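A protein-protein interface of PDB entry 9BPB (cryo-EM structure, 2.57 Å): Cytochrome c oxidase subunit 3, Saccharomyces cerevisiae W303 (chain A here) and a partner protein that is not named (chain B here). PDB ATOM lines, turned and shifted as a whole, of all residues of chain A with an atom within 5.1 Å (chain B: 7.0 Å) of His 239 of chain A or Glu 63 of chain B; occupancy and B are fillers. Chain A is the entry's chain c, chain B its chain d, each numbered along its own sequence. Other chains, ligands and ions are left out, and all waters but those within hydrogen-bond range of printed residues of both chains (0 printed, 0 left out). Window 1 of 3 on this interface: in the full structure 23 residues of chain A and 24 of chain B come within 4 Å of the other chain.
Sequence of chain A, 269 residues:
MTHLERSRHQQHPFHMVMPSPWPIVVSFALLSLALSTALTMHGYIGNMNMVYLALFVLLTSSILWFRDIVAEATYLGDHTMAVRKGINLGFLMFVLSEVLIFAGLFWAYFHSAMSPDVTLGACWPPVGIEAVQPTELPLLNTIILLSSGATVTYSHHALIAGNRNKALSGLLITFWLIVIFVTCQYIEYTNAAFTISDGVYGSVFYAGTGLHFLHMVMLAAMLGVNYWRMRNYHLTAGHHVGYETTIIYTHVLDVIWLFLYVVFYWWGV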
ATOM      1  N   ALA A  73      -3.430 -14.414  12.466  1.00  0.00           N
ATOM      2  CA  ALA A  73      -3.023 -13.189  13.137  1.00  0.00           C
ATOM      3  C   ALA A  73      -4.159 -12.537  13.910  1.00  0.00           C
ATOM      4  O   ALA A  73      -3.901 -11.813  14.878  1.00  0.00           O
ATOM      5  CB  ALA A  73      -2.465 -12.190  12.123  1.00  0.00           C
ATOM      6  N   HIS A  79       1.131 -13.636  16.158  1.00  0.00           N
ATOM      7  CA  HIS A  79       2.060 -12.562  15.810  1.00  0.00           C
ATOM      8  C   HIS A  79       2.469 -11.834  17.088  1.00  0.00           C
ATOM      9  O   HIS A  79       1.890 -10.811  17.457  1.00  0.00           O
ATOM     10  CB  HIS A  79       1.436 -11.610  14.797  1.00  0.00           C
ATOM     11  CG  HIS A  79       1.340 -12.176  13.415  1.00  0.00           C
ATOM     12  ND1 HIS A  79       1.131 -11.391  12.302  1.00  0.00           N
ATOM     13  CD2 HIS A  79       1.424 -13.450  12.966  1.00  0.00           C
ATOM     14  CE1 HIS A  79       1.091 -12.158  11.228  1.00  0.00           C
ATOM     15  NE2 HIS A  79       1.265 -13.412  11.602  1.00  0.00           N
ATOM     16  N   ARG A  84       6.325  -9.593  14.667  1.00  0.00           N
ATOM     17  CA  ARG A  84       5.924  -8.367  13.984  1.00  0.00           C
ATOM     18  C   ARG A  84       7.121  -7.595  13.448  1.00  0.00           C
ATOM     19  O   ARG A  84       6.998  -6.892  12.440  1.00  0.00           O
ATOM     20  CB  ARG A  84       5.108  -7.489  14.931  1.00  0.00           C
ATOM     21  CG  ARG A  84       3.755  -8.064  15.291  1.00  0.00           C
ATOM     22  CD  ARG A  84       3.174  -7.383  16.516  1.00  0.00           C
ATOM     23  NE  ARG A  84       3.115  -5.936  16.356  1.00  0.00           N
ATOM     24  CZ  ARG A  84       2.503  -5.116  17.198  1.00  0.00           C
ATOM     25  NH1 ARG A  84       1.886  -5.566  18.278  1.00  0.00           N
ATOM     26  NH2 ARG A  84       2.503  -3.810  16.947  1.00  0.00           N
ATOM     27  N   LEU A 235      -8.580  -4.384  12.692  1.00  0.00           N
ATOM     28  CA  LEU A 235      -7.438  -3.566  13.080  1.00  0.00           C
ATOM     29  C   LEU A 235      -7.682  -2.919  14.439  1.00  0.00           C
ATOM     30  O   LEU A 235      -8.694  -2.243  14.644  1.00  0.00           O
ATOM     31  CB  LEU A 235      -7.176  -2.490  12.031  1.00  0.00           C
ATOM     32  CG  LEU A 235      -6.897  -2.943  10.598  1.00  0.00           C
ATOM     33  CD1 LEU A 235      -6.617  -1.743   9.713  1.00  0.00           C
ATOM     34  CD2 LEU A 235      -5.738  -3.918  10.555  1.00  0.00           C
ATOM     35  N   THR A 236      -6.747  -3.119  15.363  1.00  0.00           N
ATOM     36  CA  THR A 236      -6.836  -2.556  16.700  1.00  0.00           C
ATOM     37  C   THR A 236      -6.041  -1.255  16.769  1.00  0.00           C
ATOM     38  O   THR A 236      -5.410  -0.827  15.800  1.00  0.00           O
ATOM     39  CB  THR A 236      -6.348  -3.561  17.745  1.00  0.00           C
ATOM     40  OG1 THR A 236      -4.966  -3.860  17.516  1.00  0.00           O
ATOM     41  CG2 THR A 236      -7.152  -4.846  17.662  1.00  0.00           C
ATOM     42  N   ALA A 237      -6.072  -0.618  17.938  1.00  0.00           N
ATOM     43  CA  ALA A 237      -5.442   0.685  18.107  1.00  0.00           C
ATOM     44  C   ALA A 237      -3.930   0.612  18.251  1.00  0.00           C
ATOM     45  O   ALA A 237      -3.260   1.633  18.062  1.00  0.00           O
ATOM     46  CB  ALA A 237      -6.035   1.401  19.322  1.00  0.00           C
ATOM     47  N   GLY A 238      -3.373  -0.553  18.573  1.00  0.00           N
ATOM     48  CA  GLY A 238      -1.941  -0.662  18.775  1.00  0.00           C
ATOM     49  C   GLY A 238      -1.284  -1.794  18.017  1.00  0.00           C
ATOM     50  O   GLY A 238      -0.083  -2.036  18.176  1.00  0.00           O
ATOM     51  N   HIS A 239      -2.049  -2.494  17.182  1.00  0.00           N
ATOM     52  CA  HIS A 239      -1.540  -3.650  16.443  1.00  0.00           C
ATOM     53  C   HIS A 239      -2.186  -3.642  15.062  1.00  0.00           C
ATOM     54  O   HIS A 239      -3.297  -4.148  14.886  1.00  0.00           O
ATOM     55  CB  HIS A 239      -1.828  -4.945  17.197  1.00  0.00           C
ATOM     56  CG  HIS A 239      -1.319  -6.178  16.516  1.00  0.00           C
ATOM     57  ND1 HIS A 239      -1.494  -7.439  17.043  1.00  0.00           N
ATOM     58  CD2 HIS A 239      -0.641  -6.347  15.355  1.00  0.00           C
ATOM     59  CE1 HIS A 239      -0.944  -8.330  16.239  1.00  0.00           C
ATOM     60  NE2 HIS A 239      -0.425  -7.696  15.206  1.00  0.00           N
ATOM     61  N   HIS A 240      -1.483  -3.067  14.086  1.00  0.00           N
ATOM     62  CA  HIS A 240      -1.937  -3.079  12.695  1.00  0.00           C
ATOM     63  C   HIS A 240      -0.689  -3.115  11.810  1.00  0.00           C
ATOM     64  O   HIS A 240      -0.120  -2.075  11.479  1.00  0.00           O
ATOM     65  CB  HIS A 240      -2.812  -1.873  12.387  1.00  0.00           C
ATOM     66  CG  HIS A 240      -2.371  -0.618  13.074  1.00  0.00           C
ATOM     67  ND1 HIS A 240      -1.324   0.152  12.615  1.00  0.00           N
ATOM     68  CD2 HIS A 240      -2.838   0.002  14.183  1.00  0.00           C
ATOM     69  CE1 HIS A 240      -1.163   1.191  13.415  1.00  0.00           C
ATOM     70  NE2 HIS A 240      -2.069   1.124  14.374  1.00  0.00           N
ATOM     71  N   VAL A 241      -0.282  -4.323  11.428  1.00  0.00           N
ATOM     72  CA  VAL A 241       0.881  -4.489  10.561  1.00  0.00           C
ATOM     73  C   VAL A 241       0.477  -4.469   9.094  1.00  0.00           C
ATOM     74  O   VAL A 241       1.223  -3.976   8.244  1.00  0.00           O
ATOM     75  CB  VAL A 241       1.630  -5.787  10.926  1.00  0.00           C
ATOM     76  CG1 VAL A 241       2.809  -6.010  10.000  1.00  0.00           C
ATOM     77  CG2 VAL A 241       2.093  -5.741  12.370  1.00  0.00           C
ATOM     78  N   THR B  33     -11.704 -13.933  31.249  1.00  0.00           N
ATOM     79  CA  THR B  33     -10.372 -13.522  30.830  1.00  0.00           C
ATOM     80  C   THR B  33      -9.470 -13.352  32.050  1.00  0.00           C
ATOM     81  O   THR B  33      -9.912 -12.937  33.124  1.00  0.00           O
ATOM     82  CB  THR B  33     -10.451 -12.221  30.029  1.00  0.00           C
ATOM     83  OG1 THR B  33     -11.318 -12.411  28.904  1.00  0.00           O
ATOM     84  CG2 THR B  33      -9.082 -11.815  29.515  1.00  0.00           C
ATOM     85  N   LEU B  46      -6.919 -16.255  28.170  1.00  0.00           N
ATOM     86  CA  LEU B  46      -6.348 -15.058  27.499  1.00  0.00           C
ATOM     87  C   LEU B  46      -7.435 -14.348  26.676  1.00  0.00           C
ATOM     88  O   LEU B  46      -7.529 -13.122  26.823  1.00  0.00           O
ATOM     89  CB  LEU B  46      -5.156 -15.493  26.641  1.00  0.00           C
ATOM     90  CG  LEU B  46      -3.917 -15.904  27.435  1.00  0.00           C
ATOM     91  CD1 LEU B  46      -2.736 -16.172  26.517  1.00  0.00           C
ATOM     92  CD2 LEU B  46      -3.560 -14.839  28.460  1.00  0.00           C
ATOM     93  N   ILE B  47      -8.284 -15.077  25.937  1.00  0.00           N
ATOM     94  CA  ILE B  47      -9.347 -14.450  25.080  1.00  0.00           C
ATOM     95  C   ILE B  47      -9.972 -13.286  25.856  1.00  0.00           C
ATOM     96  O   ILE B  47     -10.159 -13.438  27.086  1.00  0.00           O
ATOM     97  CB  ILE B  47     -10.403 -15.476  24.608  1.00  0.00           C
ATOM     98  CG1 ILE B  47     -11.538 -15.660  25.619  1.00  0.00           C
ATOM     99  CG2 ILE B  47      -9.747 -16.802  24.254  1.00  0.00           C
ATOM    100  CD1 ILE B  47     -12.560 -16.690  25.208  1.00  0.00           C
ATOM    101  N   GLY B  48     -10.367 -12.207  25.175  1.00  0.00           N
ATOM    102  CA  GLY B  48     -10.813 -11.019  25.862  1.00  0.00           C
ATOM    103  C   GLY B  48     -12.199 -10.578  25.447  1.00  0.00           C
ATOM    104  O   GLY B  48     -12.843 -11.190  24.590  1.00  0.00           O
ATOM    105  N   PRO B  49     -12.695  -9.509  26.065  1.00  0.00           N
ATOM    106  CA  PRO B  49     -13.987  -8.957  25.648  1.00  0.00           C
ATOM    107  C   PRO B  49     -13.833  -8.092  24.408  1.00  0.00           C
ATOM    108  O   PRO B  49     -12.920  -7.269  24.313  1.00  0.00           O
ATOM    109  CB  PRO B  49     -14.424  -8.129  26.860  1.00  0.00           C
ATOM    110  CG  PRO B  49     -13.141  -7.708  27.485  1.00  0.00           C
ATOM    111  CD  PRO B  49     -12.170  -8.838  27.266  1.00  0.00           C
ATOM    112  N   PRO B  57     -11.044  -0.738  18.573  1.00  0.00           N
ATOM    113  CA  PRO B  57     -10.628  -1.769  19.528  1.00  0.00           C
ATOM    114  C   PRO B  57      -9.232  -1.508  20.072  1.00  0.00           C
ATOM    115  O   PRO B  57      -8.373  -0.949  19.389  1.00  0.00           O
ATOM    116  CB  PRO B  57     -10.666  -3.060  18.699  1.00  0.00           C
ATOM    117  CG  PRO B  57     -11.496  -2.729  17.495  1.00  0.00           C
ATOM    118  CD  PRO B  57     -11.233  -1.287  17.222  1.00  0.00           C
ATOM    119  N   THR B  58      -9.018  -1.918  21.317  1.00  0.00           N
ATOM    120  CA  THR B  58      -7.705  -1.857  21.937  1.00  0.00           C
ATOM    121  C   THR B  58      -7.103  -3.256  22.032  1.00  0.00           C
ATOM    122  O   THR B  58      -7.773  -4.266  21.810  1.00  0.00           O
ATOM    123  CB  THR B  58      -7.788  -1.214  23.323  1.00  0.00           C
ATOM    124  OG1 THR B  58      -8.868  -1.800  24.060  1.00  0.00           O
ATOM    125  CG2 THR B  58      -8.018   0.282  23.207  1.00  0.00           C
ATOM    126  N   ASP B  59      -5.812  -3.308  22.366  1.00  0.00           N
ATOM    127  CA  ASP B  59      -5.135  -4.597  22.476  1.00  0.00           C
ATOM    128  C   ASP B  59      -5.659  -5.398  23.659  1.00  0.00           C
ATOM    129  O   ASP B  59      -5.737  -6.629  23.595  1.00  0.00           O
ATOM    130  CB  ASP B  59      -3.626  -4.390  22.587  1.00  0.00           C
ATOM    131  CG  ASP B  59      -3.022  -3.837  21.316  1.00  0.00           C
ATOM    132  OD1 ASP B  59      -3.619  -4.043  20.240  1.00  0.00           O
ATOM    133  OD2 ASP B  59      -1.951  -3.201  21.391  1.00  0.00           O
ATOM    134  N   LEU B  60      -6.036  -4.720  24.744  1.00  0.00           N
ATOM    135  CA  LEU B  60      -6.622  -5.428  25.876  1.00  0.00           C
ATOM    136  C   LEU B  60      -8.019  -5.943  25.565  1.00  0.00           C
ATOM    137  O   LEU B  60      -8.584  -6.694  26.365  1.00  0.00           O
ATOM    138  CB  LEU B  60      -6.658  -4.521  27.107  1.00  0.00           C
ATOM    139  CG  LEU B  60      -5.361  -4.454  27.913  1.00  0.00           C
ATOM    140  CD1 LEU B  60      -5.454  -3.400  29.003  1.00  0.00           C
ATOM    141  CD2 LEU B  60      -5.034  -5.812  28.507  1.00  0.00           C
ATOM    142  N   ASP B  61      -8.588  -5.552  24.423  1.00  0.00           N
ATOM    143  CA  ASP B  61      -9.904  -6.045  24.037  1.00  0.00           C
ATOM    144  C   ASP B  61      -9.803  -7.263  23.125  1.00  0.00           C
ATOM    145  O   ASP B  61     -10.495  -8.263  23.339  1.00  0.00           O
ATOM    146  CB  ASP B  61     -10.699  -4.936  23.351  1.00  0.00           C
ATOM    147  CG  ASP B  61     -11.136  -3.851  24.311  1.00  0.00           C
ATOM    148  OD1 ASP B  61     -11.289  -4.150  25.514  1.00  0.00           O
ATOM    149  OD2 ASP B  61     -11.327  -2.702  23.865  1.00  0.00           O
ATOM    150  N   GLN B  62      -8.945  -7.204  22.107  1.00  0.00           N
ATOM    151  CA  GLN B  62      -8.965  -8.190  21.035  1.00  0.00           C
ATOM    152  C   GLN B  62      -7.606  -8.846  20.798  1.00  0.00           C
ATOM    153  O   GLN B  62      -7.173  -8.991  19.654  1.00  0.00           O
ATOM    154  CB  GLN B  62      -9.482  -7.556  19.744  1.00  0.00           C
ATOM    155  CG  GLN B  62     -10.968  -7.760  19.524  1.00  0.00           C
ATOM    156  CD  GLN B  62     -11.531  -6.841  18.461  1.00  0.00           C
ATOM    157  OE1 GLN B  62     -10.786  -6.166  17.752  1.00  0.00           O
ATOM    158  NE2 GLN B  62     -12.851  -6.806  18.350  1.00  0.00           N
ATOM    159  N   GLU B  63      -6.921  -9.244  21.865  1.00  0.00           N
ATOM    160  CA  GLU B  63      -5.805 -10.172  21.749  1.00  0.00           C
ATOM    161  C   GLU B  63      -6.273 -11.555  22.182  1.00  0.00           C
ATOM    162  O   GLU B  63      -7.186 -11.687  23.001  1.00  0.00           O
ATOM    163  CB  GLU B  63      -4.614  -9.718  22.593  1.00  0.00           C
ATOM    164  CG  GLU B  63      -3.844  -8.537  22.019  1.00  0.00           C
ATOM    165  CD  GLU B  63      -3.094  -8.874  20.745  1.00  0.00           C
ATOM    166  OE1 GLU B  63      -2.688 -10.042  20.579  1.00  0.00           O
ATOM    167  OE2 GLU B  63      -2.911  -7.968  19.907  1.00  0.00           O
ATOM    168  N   THR B  64      -5.659 -12.595  21.614  1.00  0.00           N
ATOM    169  CA  THR B  64      -6.192 -13.940  21.798  1.00  0.00           C
ATOM    170  C   THR B  64      -5.188 -15.012  22.203  1.00  0.00           C
ATOM    171  O   THR B  64      -5.600 -15.986  22.842  1.00  0.00           O
ATOM    172  CB  THR B  64      -6.908 -14.407  20.521  1.00  0.00           C
ATOM    173  OG1 THR B  64      -7.438 -15.722  20.725  1.00  0.00           O
ATOM    174  CG2 THR B  64      -5.958 -14.418  19.340  1.00  0.00           C
ATOM    175  N   GLY B  65      -3.907 -14.883  21.870  1.00  0.00           N
ATOM    176  CA  GLY B  65      -3.011 -16.005  22.078  1.00  0.00           C
ATOM    177  C   GLY B  65      -1.671 -15.680  22.697  1.00  0.00           C
ATOM    178  O   GLY B  65      -1.595 -14.947  23.688  1.00  0.00           O
ATOM    179  N   LEU B  66      -0.601 -16.237  22.121  1.00  0.00           N
ATOM    180  CA  LEU B  66       0.740 -15.986  22.636  1.00  0.00           C
ATOM    181  C   LEU B  66       1.098 -14.509  22.565  1.00  0.00           C
ATOM    182  O   LEU B  66       1.917 -14.032  23.355  1.00  0.00           O
ATOM    183  CB  LEU B  66       1.759 -16.824  21.863  1.00  0.00           C
ATOM    184  CG  LEU B  66       3.204 -16.824  22.362  1.00  0.00           C
ATOM    185  CD1 LEU B  66       3.326 -17.597  23.660  1.00  0.00           C
ATOM    186  CD2 LEU B  66       4.122 -17.407  21.305  1.00  0.00           C
ATOM    187  N   ALA B  67       0.497 -13.773  21.629  1.00  0.00           N
ATOM    188  CA  ALA B  67       0.687 -12.328  21.599  1.00  0.00           C
ATOM    189  C   ALA B  67       0.045 -11.665  22.812  1.00  0.00           C
ATOM    190  O   ALA B  67       0.523 -10.628  23.285  1.00  0.00           O
ATOM    191  CB  ALA B  67       0.120 -11.752  20.304  1.00  0.00           C
ATOM    192  N   ARG B  68      -1.045 -12.243  23.323  1.00  0.00           N
ATOM    193  CA  ARG B  68      -1.691 -11.682  24.505  1.00  0.00           C
ATOM    194  C   ARG B  68      -0.906 -11.999  25.771  1.00  0.00           C
ATOM    195  O   ARG B  68      -0.807 -11.158  26.671  1.00  0.00           O
ATOM    196  CB  ARG B  68      -3.121 -12.202  24.627  1.00  0.00           C
ATOM    197  CG  ARG B  68      -3.870 -11.613  25.805  1.00  0.00           C
ATOM    198  CD  ARG B  68      -5.367 -11.690  25.617  1.00  0.00           C
ATOM    199  NE  ARG B  68      -6.083 -11.085  26.733  1.00  0.00           N
ATOM    200  CZ  ARG B  68      -6.904 -10.051  26.619  1.00  0.00           C
ATOM    201  NH1 ARG B  68      -7.146  -9.486  25.450  1.00  0.00           N
ATOM    202  NH2 ARG B  68      -7.494  -9.568  27.708  1.00  0.00           N
ATOM    203  N   LEU B  69      -0.352 -13.210  25.863  1.00  0.00           N
ATOM    204  CA  LEU B  69       0.426 -13.573  27.042  1.00  0.00           C
ATOM    205  C   LEU B  69       1.648 -12.677  27.184  1.00  0.00           C
ATOM    206  O   LEU B  69       2.012 -12.282  28.298  1.00  0.00           O
ATOM    207  CB  LEU B  69       0.835 -15.043  26.966  1.00  0.00           C
ATOM    208  CG  LEU B  69       1.308 -15.713  28.256  1.00  0.00           C
ATOM    209  CD1 LEU B  69       0.868 -17.161  28.282  1.00  0.00           C
ATOM    210  CD2 LEU B  69       2.815 -15.625  28.399  1.00  0.00           C
ATOM    211  N   LEU B  71       1.710  -9.600  26.041  1.00  0.00           N
ATOM    212  CA  LEU B  71       1.163  -8.296  26.401  1.00  0.00           C
ATOM    213  C   LEU B  71       0.847  -8.220  27.888  1.00  0.00           C
ATOM    214  O   LEU B  71       1.074  -7.186  28.526  1.00  0.00           O
ATOM    215  CB  LEU B  71      -0.084  -8.004  25.567  1.00  0.00           C
ATOM    216  CG  LEU B  71      -0.986  -6.861  26.036  1.00  0.00           C
ATOM    217  CD1 LEU B  71      -0.346  -5.517  25.728  1.00  0.00           C
ATOM    218  CD2 LEU B  71      -2.354  -6.964  25.391  1.00  0.00           C
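The side-chain hydroxyl (OG1) of Thr 236 of chain A is in hydrogen-bond range of the side-chain carboxylate (OD1) of Asp 59 of chain B. OE2 of Glu 63 of chain B is in hydrogen-bond range of ND1 of His 239 of chain A, 3.2 Å away. N of Ala 237 of chain A is in hydrogen-bond range of O of Pro 57 of chain B (2.7 Å).
Printed residues of chain B within 4 Å of Thr 236 of chain A: Pro 57 (3.5 Å), Asp 59 (3.0 Å) and Gln 62 (3.9 Å). Gly 238 of chain A touches just one residue of chain B: Asp 59. His 239 of chain A touches just these residues of chain B: Asp 59 and Glu 63. His 240 of chain A touches none of the printed residues of chain B. Thr 33 of chain B touches none of the printed residues of chain A. Of the printed residues of chain A, Pro 57 of chain B touches Leu 235, Thr 236 and Ala 237. Printed residues of chain A within 4 Å of Gln 62 of chain B: Thr 236. Of the printed residues of chain A, Glu 63 of chain B touches His 239. The nearest printed residue of chain A that does not touch Glu 63 of chain B is Thr 236 of chain A (5.2 Å). The nearest printed residue of chain A that does not touch Pro 57 of chain B is Gly 238 of chain A (5.1 Å).
Hydrophobic or aromatic side chains of chain B within 4 Å of the printed part of chain A: Pro 57 and Ala 67. Among the printed residues, no Asp or Glu carboxylate lies within 4 Å of a Lys or Arg side-chain nitrogen of the other chain.
Among the printed residues, pairs that only touch across the chains: His 79 of chain A with Ala 67 of chain B (3.5 Å), Leu 235 of chain A with Pro 57 of chain B (3.7 Å), Thr 236 of chain A with Pro 57 of chain B (3.5 Å), Thr 236 of chain A with Gln 62 of chain B (3.9 Å), Gly 238 of chain A with Asp 59 of chain B (3.6 Å) and His 239 of chain A with Asp 59 of chain B (3.6 Å).
OG1 of Thr 236 of chain A lies within hydrogen-bond range of O of His 239 of chain A. The backbone carbonyl oxygen of Glu 63 of chain B sits close to the guanidinium group of Arg 68 of chain B (3.3 Å). O of Gly 238 of chain A is in hydrogen-bond range of NH2 of Arg 84 of chain A.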
